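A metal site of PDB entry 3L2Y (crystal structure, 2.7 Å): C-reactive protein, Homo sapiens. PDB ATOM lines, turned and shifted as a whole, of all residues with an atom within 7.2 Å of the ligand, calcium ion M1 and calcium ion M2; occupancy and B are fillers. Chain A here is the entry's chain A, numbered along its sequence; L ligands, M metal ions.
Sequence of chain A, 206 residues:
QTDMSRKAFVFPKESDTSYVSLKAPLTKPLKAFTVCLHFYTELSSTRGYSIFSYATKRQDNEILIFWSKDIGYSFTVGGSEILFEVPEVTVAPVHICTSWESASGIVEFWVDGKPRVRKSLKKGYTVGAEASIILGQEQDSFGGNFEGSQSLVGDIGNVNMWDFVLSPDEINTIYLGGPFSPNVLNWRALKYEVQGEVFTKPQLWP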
ATOM      1  N   TYR A  49      11.031   8.383  -2.956  1.00  0.00           N
ATOM      2  CA  TYR A  49      12.150   8.235  -3.876  1.00  0.00           C
ATOM      3  C   TYR A  49      11.772   7.497  -5.154  1.00  0.00           C
ATOM      4  O   TYR A  49      10.822   6.704  -5.162  1.00  0.00           O
ATOM      5  CB  TYR A  49      13.332   7.518  -3.221  1.00  0.00           C
ATOM      6  CG  TYR A  49      12.979   6.202  -2.590  1.00  0.00           C
ATOM      7  CD1 TYR A  49      13.092   5.020  -3.295  1.00  0.00           C
ATOM      8  CD2 TYR A  49      12.562   6.142  -1.275  1.00  0.00           C
ATOM      9  CE1 TYR A  49      12.779   3.804  -2.702  1.00  0.00           C
ATOM     10  CE2 TYR A  49      12.249   4.943  -0.682  1.00  0.00           C
ATOM     11  CZ  TYR A  49      12.346   3.775  -1.400  1.00  0.00           C
ATOM     12  OH  TYR A  49      12.020   2.581  -0.789  1.00  0.00           O
ATOM     13  N   SER A  50      12.513   7.774  -6.233  1.00  0.00           N
ATOM     14  CA  SER A  50      12.305   7.115  -7.514  1.00  0.00           C
ATOM     15  C   SER A  50      13.133   5.834  -7.633  1.00  0.00           C
ATOM     16  O   SER A  50      14.350   5.829  -7.423  1.00  0.00           O
ATOM     17  CB  SER A  50      12.630   8.073  -8.668  1.00  0.00           C
ATOM     18  OG  SER A  50      12.821   7.364  -9.875  1.00  0.00           O
ATOM     19  N   SER A  53      12.824   5.372 -13.433  1.00  0.00           N
ATOM     20  CA  SER A  53      12.204   6.476 -14.178  1.00  0.00           C
ATOM     21  C   SER A  53      12.379   6.360 -15.689  1.00  0.00           C
ATOM     22  O   SER A  53      13.500   6.369 -16.196  1.00  0.00           O
ATOM     23  CB  SER A  53      12.747   7.840 -13.727  1.00  0.00           C
ATOM     24  OG  SER A  53      12.065   8.898 -14.387  1.00  0.00           O
ATOM     25  N   GLN A  59       6.041  12.708 -22.195  1.00  0.00           N
ATOM     26  CA  GLN A  59       5.611  12.318 -20.852  1.00  0.00           C
ATOM     27  C   GLN A  59       6.803  11.962 -19.967  1.00  0.00           C
ATOM     28  O   GLN A  59       7.525  10.999 -20.231  1.00  0.00           O
ATOM     29  CB  GLN A  59       4.636  11.137 -20.941  1.00  0.00           C
ATOM     30  CG  GLN A  59       4.261  10.549 -19.609  1.00  0.00           C
ATOM     31  CD  GLN A  59       3.420  11.482 -18.787  1.00  0.00           C
ATOM     32  OE1 GLN A  59       3.843  11.970 -17.746  1.00  0.00           O
ATOM     33  NE2 GLN A  59       2.199  11.742 -19.256  1.00  0.00           N
ATOM     34  N   ASP A  60       7.003  12.745 -18.907  1.00  0.00           N
ATOM     35  CA  ASP A  60       8.115  12.516 -17.989  1.00  0.00           C
ATOM     36  C   ASP A  60       7.933  11.247 -17.155  1.00  0.00           C
ATOM     37  O   ASP A  60       8.899  10.635 -16.729  1.00  0.00           O
ATOM     38  CB  ASP A  60       8.341  13.744 -17.099  1.00  0.00           C
ATOM     39  CG  ASP A  60       7.125  14.100 -16.232  1.00  0.00           C
ATOM     40  OD1 ASP A  60       5.974  13.965 -16.693  1.00  0.00           O
ATOM     41  OD2 ASP A  60       7.332  14.543 -15.088  1.00  0.00           O
ATOM     42  N   ASN A  61       6.678  10.850 -16.965  1.00  0.00           N
ATOM     43  CA  ASN A  61       6.361   9.658 -16.210  1.00  0.00           C
ATOM     44  C   ASN A  61       5.698   8.605 -17.068  1.00  0.00           C
ATOM     45  O   ASN A  61       4.582   8.164 -16.771  1.00  0.00           O
ATOM     46  CB  ASN A  61       5.477  10.034 -15.023  1.00  0.00           C
ATOM     47  CG  ASN A  61       6.161  11.030 -14.097  1.00  0.00           C
ATOM     48  OD1 ASN A  61       7.305  11.402 -14.323  1.00  0.00           O
ATOM     49  ND2 ASN A  61       5.468  11.450 -13.063  1.00  0.00           N
ATOM     50  N   LEU A  64       6.881   4.807 -14.358  1.00  0.00           N
ATOM     51  CA  LEU A  64       7.531   5.232 -13.117  1.00  0.00           C
ATOM     52  C   LEU A  64       7.230   4.319 -11.942  1.00  0.00           C
ATOM     53  O   LEU A  64       6.086   4.182 -11.524  1.00  0.00           O
ATOM     54  CB  LEU A  64       7.157   6.670 -12.747  1.00  0.00           C
ATOM     55  CG  LEU A  64       7.793   7.126 -11.441  1.00  0.00           C
ATOM     56  CD1 LEU A  64       9.308   7.198 -11.574  1.00  0.00           C
ATOM     57  CD2 LEU A  64       7.243   8.467 -10.977  1.00  0.00           C
ATOM     58  N   PHE A  66       7.974   4.141  -8.083  1.00  0.00           N
ATOM     59  CA  PHE A  66       8.308   5.160  -7.102  1.00  0.00           C
ATOM     60  C   PHE A  66       7.832   4.732  -5.720  1.00  0.00           C
ATOM     61  O   PHE A  66       6.819   4.041  -5.587  1.00  0.00           O
ATOM     62  CB  PHE A  66       7.597   6.433  -7.506  1.00  0.00           C
ATOM     63  CG  PHE A  66       8.003   7.639  -6.730  1.00  0.00           C
ATOM     64  CD1 PHE A  66       9.040   8.438  -7.179  1.00  0.00           C
ATOM     65  CD2 PHE A  66       7.314   8.016  -5.588  1.00  0.00           C
ATOM     66  CE1 PHE A  66       9.410   9.585  -6.486  1.00  0.00           C
ATOM     67  CE2 PHE A  66       7.683   9.158  -4.887  1.00  0.00           C
ATOM     68  CZ  PHE A  66       8.727   9.934  -5.343  1.00  0.00           C
ATOM     69  N   TRP A  67       8.568   5.107  -4.685  1.00  0.00           N
ATOM     70  CA  TRP A  67       8.111   4.854  -3.330  1.00  0.00           C
ATOM     71  C   TRP A  67       7.649   6.176  -2.773  1.00  0.00           C
ATOM     72  O   TRP A  67       8.431   7.122  -2.676  1.00  0.00           O
ATOM     73  CB  TRP A  67       9.245   4.308  -2.453  1.00  0.00           C
ATOM     74  CG  TRP A  67       8.819   4.201  -1.021  1.00  0.00           C
ATOM     75  CD1 TRP A  67       8.917   5.172  -0.056  1.00  0.00           C
ATOM     76  CD2 TRP A  67       8.203   3.084  -0.394  1.00  0.00           C
ATOM     77  NE1 TRP A  67       8.399   4.711   1.135  1.00  0.00           N
ATOM     78  CE2 TRP A  67       7.955   3.432   0.951  1.00  0.00           C
ATOM     79  CE3 TRP A  67       7.839   1.810  -0.829  1.00  0.00           C
ATOM     80  CZ2 TRP A  67       7.361   2.564   1.843  1.00  0.00           C
ATOM     81  CZ3 TRP A  67       7.253   0.953   0.058  1.00  0.00           C
ATOM     82  CH2 TRP A  67       7.009   1.325   1.384  1.00  0.00           C
ATOM     83  N   SER A  68       6.372   6.266  -2.416  1.00  0.00           N
ATOM     84  CA  SER A  68       5.885   7.505  -1.821  1.00  0.00           C
ATOM     85  C   SER A  68       5.702   7.365  -0.297  1.00  0.00           C
ATOM     86  O   SER A  68       5.179   6.350   0.182  1.00  0.00           O
ATOM     87  CB  SER A  68       4.632   8.036  -2.543  1.00  0.00           C
ATOM     88  OG  SER A  68       3.510   7.258  -2.224  1.00  0.00           O
ATOM     89  N   SER A  74       4.268   3.295  -5.680  1.00  0.00           N
ATOM     90  CA  SER A  74       3.450   3.989  -6.663  1.00  0.00           C
ATOM     91  C   SER A  74       3.886   3.584  -8.060  1.00  0.00           C
ATOM     92  O   SER A  74       5.065   3.664  -8.412  1.00  0.00           O
ATOM     93  CB  SER A  74       3.569   5.497  -6.479  1.00  0.00           C
ATOM     94  OG  SER A  74       3.818   6.126  -7.726  1.00  0.00           O
ATOM     95  N   THR A  76       3.301   4.190 -12.118  1.00  0.00           N
ATOM     96  CA  THR A  76       2.744   5.128 -13.070  1.00  0.00           C
ATOM     97  C   THR A  76       3.010   4.717 -14.520  1.00  0.00           C
ATOM     98  O   THR A  76       4.142   4.423 -14.901  1.00  0.00           O
ATOM     99  CB  THR A  76       3.307   6.541 -12.840  1.00  0.00           C
ATOM    100  OG1 THR A  76       3.162   6.902 -11.455  1.00  0.00           O
ATOM    101  CG2 THR A  76       2.587   7.545 -13.722  1.00  0.00           C
ATOM    102  N   GLU A  81      -1.400   7.189 -12.199  1.00  0.00           N
ATOM    103  CA  GLU A  81      -0.793   6.545 -11.051  1.00  0.00           C
ATOM    104  C   GLU A  81      -1.769   5.618 -10.350  1.00  0.00           C
ATOM    105  O   GLU A  81      -2.937   5.962 -10.184  1.00  0.00           O
ATOM    106  CB  GLU A  81      -0.301   7.619 -10.067  1.00  0.00           C
ATOM    107  CG  GLU A  81       0.348   7.111  -8.799  1.00  0.00           C
ATOM    108  CD  GLU A  81       0.650   8.216  -7.797  1.00  0.00           C
ATOM    109  OE1 GLU A  81      -0.288   8.981  -7.479  1.00  0.00           O
ATOM    110  OE2 GLU A  81       1.814   8.334  -7.339  1.00  0.00           O
ATOM    111  N   GLU A 138      14.622  11.066 -10.348  1.00  0.00           N
ATOM    112  CA  GLU A 138      13.289  11.062 -10.929  1.00  0.00           C
ATOM    113  C   GLU A 138      13.248  12.162 -11.982  1.00  0.00           C
ATOM    114  O   GLU A 138      13.580  13.315 -11.708  1.00  0.00           O
ATOM    115  CB  GLU A 138      12.221  11.299  -9.864  1.00  0.00           C
ATOM    116  CG  GLU A 138      10.817  10.777 -10.214  1.00  0.00           C
ATOM    117  CD  GLU A 138      10.137  11.581 -11.315  1.00  0.00           C
ATOM    118  OE1 GLU A 138      10.107  12.817 -11.183  1.00  0.00           O
ATOM    119  OE2 GLU A 138       9.653  10.982 -12.313  1.00  0.00           O
ATOM    120  N   GLN A 139      12.870  11.791 -13.206  1.00  0.00           N
ATOM    121  CA  GLN A 139      12.841  12.722 -14.333  1.00  0.00           C
ATOM    122  C   GLN A 139      11.583  13.567 -14.371  1.00  0.00           C
ATOM    123  O   GLN A 139      10.473  13.042 -14.287  1.00  0.00           O
ATOM    124  CB  GLN A 139      12.929  11.946 -15.637  1.00  0.00           C
ATOM    125  CG  GLN A 139      14.307  11.449 -15.974  1.00  0.00           C
ATOM    126  CD  GLN A 139      14.287  10.484 -17.136  1.00  0.00           C
ATOM    127  OE1 GLN A 139      14.875  10.756 -18.191  1.00  0.00           O
ATOM    128  NE2 GLN A 139      13.590   9.364 -16.958  1.00  0.00           N
ATOM    129  N   ASP A 140      11.752  14.876 -14.510  1.00  0.00           N
ATOM    130  CA  ASP A 140      10.622  15.756 -14.753  1.00  0.00           C
ATOM    131  C   ASP A 140      10.637  16.267 -16.188  1.00  0.00           C
ATOM    132  O   ASP A 140       9.711  16.922 -16.648  1.00  0.00           O
ATOM    133  CB  ASP A 140      10.636  16.930 -13.782  1.00  0.00           C
ATOM    134  CG  ASP A 140      10.026  16.577 -12.455  1.00  0.00           C
ATOM    135  OD1 ASP A 140       9.302  15.557 -12.399  1.00  0.00           O
ATOM    136  OD2 ASP A 140      10.246  17.313 -11.474  1.00  0.00           O
ATOM    137  N   SER A 141      11.713  15.950 -16.906  1.00  0.00           N
ATOM    138  CA  SER A 141      11.817  16.279 -18.306  1.00  0.00           C
ATOM    139  C   SER A 141      12.597  15.167 -18.956  1.00  0.00           C
ATOM    140  O   SER A 141      13.234  14.374 -18.269  1.00  0.00           O
ATOM    141  CB  SER A 141      12.536  17.614 -18.492  1.00  0.00           C
ATOM    142  OG  SER A 141      13.928  17.469 -18.297  1.00  0.00           O
ATOM    143  N   GLY A 144      16.281  14.793 -17.703  1.00  0.00           N
ATOM    144  CA  GLY A 144      16.711  15.734 -16.692  1.00  0.00           C
ATOM    145  C   GLY A 144      15.635  16.311 -15.789  1.00  0.00           C
ATOM    146  O   GLY A 144      14.549  15.727 -15.612  1.00  0.00           O
ATOM    147  N   ASN A 145      15.948  17.473 -15.220  1.00  0.00           N
ATOM    148  CA  ASN A 145      15.070  18.126 -14.262  1.00  0.00           C
ATOM    149  C   ASN A 145      14.808  17.250 -13.060  1.00  0.00           C
ATOM    150  O   ASN A 145      13.658  16.925 -12.756  1.00  0.00           O
ATOM    151  CB  ASN A 145      13.762  18.565 -14.898  1.00  0.00           C
ATOM    152  CG  ASN A 145      13.890  19.904 -15.566  1.00  0.00           C
ATOM    153  OD1 ASN A 145      13.679  20.027 -16.778  1.00  0.00           O
ATOM    154  ND2 ASN A 145      14.258  20.914 -14.804  1.00  0.00           N
ATOM    155  N   PHE A 146      15.880  16.886 -12.377  1.00  0.00           N
ATOM    156  CA  PHE A 146      15.811  16.001 -11.229  1.00  0.00           C
ATOM    157  C   PHE A 146      15.463  16.783  -9.971  1.00  0.00           C
ATOM    158  O   PHE A 146      15.769  17.966  -9.878  1.00  0.00           O
ATOM    159  CB  PHE A 146      17.156  15.308 -11.049  1.00  0.00           C
ATOM    160  CG  PHE A 146      17.662  14.656 -12.306  1.00  0.00           C
ATOM    161  CD1 PHE A 146      16.842  13.812 -13.043  1.00  0.00           C
ATOM    162  CD2 PHE A 146      18.944  14.886 -12.766  1.00  0.00           C
ATOM    163  CE1 PHE A 146      17.309  13.218 -14.197  1.00  0.00           C
ATOM    164  CE2 PHE A 146      19.412  14.286 -13.912  1.00  0.00           C
ATOM    165  CZ  PHE A 146      18.594  13.446 -14.632  1.00  0.00           C
ATOM    166  N   GLU A 147      14.806  16.126  -9.017  1.00  0.00           N
ATOM    167  CA  GLU A 147      14.569  16.695  -7.700  1.00  0.00           C
ATOM    168  C   GLU A 147      15.331  15.862  -6.696  1.00  0.00           C
ATOM    169  O   GLU A 147      15.208  14.634  -6.663  1.00  0.00           O
ATOM    170  CB  GLU A 147      13.079  16.682  -7.327  1.00  0.00           C
ATOM    171  CG  GLU A 147      12.127  17.442  -8.242  1.00  0.00           C
ATOM    172  CD  GLU A 147      10.710  17.564  -7.650  1.00  0.00           C
ATOM    173  OE1 GLU A 147      10.577  18.194  -6.578  1.00  0.00           O
ATOM    174  OE2 GLU A 147       9.736  17.035  -8.243  1.00  0.00           O
ATOM    175  N   GLN A 150      13.801  13.411  -4.295  1.00  0.00           N
ATOM    176  CA  GLN A 150      13.242  12.201  -4.891  1.00  0.00           C
ATOM    177  C   GLN A 150      14.320  11.230  -5.352  1.00  0.00           C
ATOM    178  O   GLN A 150      14.022  10.216  -5.982  1.00  0.00           O
ATOM    179  CB  GLN A 150      12.319  12.561  -6.058  1.00  0.00           C
ATOM    180  CG  GLN A 150      11.046  13.240  -5.608  1.00  0.00           C
ATOM    181  CD  GLN A 150      10.110  13.512  -6.755  1.00  0.00           C
ATOM    182  OE1 GLN A 150      10.563  13.680  -7.869  1.00  0.00           O
ATOM    183  NE2 GLN A 150       8.808  13.533  -6.490  1.00  0.00           N
HETATM  184  C1  LIG L   1       6.061  11.512  -9.224  1.00  0.00           C
HETATM  185  C2  LIG L   1       5.957  10.509  -8.130  1.00  0.00           C
HETATM  186  O1  LIG L   1       6.688  13.207 -11.323  1.00  0.00           O
HETATM  187  O2  LIG L   1       7.818  14.720  -9.903  1.00  0.00           O
HETATM  188  O3  LIG L   1       5.337  14.745 -10.033  1.00  0.00           O
HETATM  189  O4  LIG L   1       6.582  12.805  -8.920  1.00  0.00           O
HETATM  190  N1  LIG L   1       4.743  10.520  -7.299  1.00  0.00           N
HETATM  191  P1  LIG L   1       6.563  13.921 -10.040  1.00  0.00           P
HETATM  192 CA    CA M   1      10.046  15.119 -10.021  1.00  0.00          CA
HETATM  193 CA    CA M   2       8.380  13.202 -13.026  1.00  0.00          CA
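OE2 of Glu 81 is in salt-bridge range of N1 of the ligand (3.7 Å).
The side-chain hydroxyl of Ser 53 is in hydrogen-bond range of the side-chain amide nitrogen of Gln 139 (3.0 Å). The backbone NH (N) of Asn 61 lies within hydrogen-bond range of the side-chain amide oxygen (OE1) of Gln 59 (3.1 Å). The backbone NH (N) of Asp 140 lies close to the backbone carbonyl oxygen (O) of Asn 145, 3.3 Å away. N of Ser 50 sits at hydrogen-bond distance from O of Gln 150, 2.9 Å away. The side-chain amide oxygen (OE1) of Gln 59 sits close to the side-chain carboxylate (OD1) of Asp 60. The side-chain hydroxyl of Ser 74 is in hydrogen-bond range of the side-chain carboxylate of Glu 81. N of Leu 64 sits at hydrogen-bond distance from O of Thr 76 (2.8 Å). The backbone NH (N) of Ser 74 lies within hydrogen-bond range of the backbone carbonyl oxygen (O) of Phe 66 (2.7 Å).
Leu 64 touches the ligand (CD2 to C1, 3.7 Å). Phe 66 touches the ligand. Hydrophobic or aromatic side chains within 4 Å of the ligand: Leu 64 and Phe 66. Of the 22 residues printed, 8 come within 4 Å of the ligand. The nearest printed residue that does not touch the ligand is Asp 60 (4.05 Å).
Within 4 Å of calcium ion M1: Glu 138, Asp 140, Glu 147 and Gln 150.
Within 4 Å of calcium ion M2: Asp 60, Asn 61, Glu 138, Gln 139 and Asp 140. Along chain A the residues within 4 Å of calcium ion M2 span positions 60 to 140.
Calcium ion M1 is bound by O2 of the ligand, OD1 of Asp 140, OE1 of Glu 138, OE2 of Glu 147, OD2 of Asp 140 and OE1 of Gln 150. Calcium ion M1 has six donor atoms within binding distance.
Calcium ion M2 is bound by O1 of the ligand (2.4 Å), O of Gln 139 (2.4 Å), OD1 of Asn 61 (2.5 Å), OE1 of Glu 138 (2.6 Å), OD1 of Asp 140 (2.6 Å), OE2 of Glu 138 (2.7 Å) and OD2 of Asp 60 (2.7 Å). Calcium ion M2 has seven donor atoms within binding distance.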
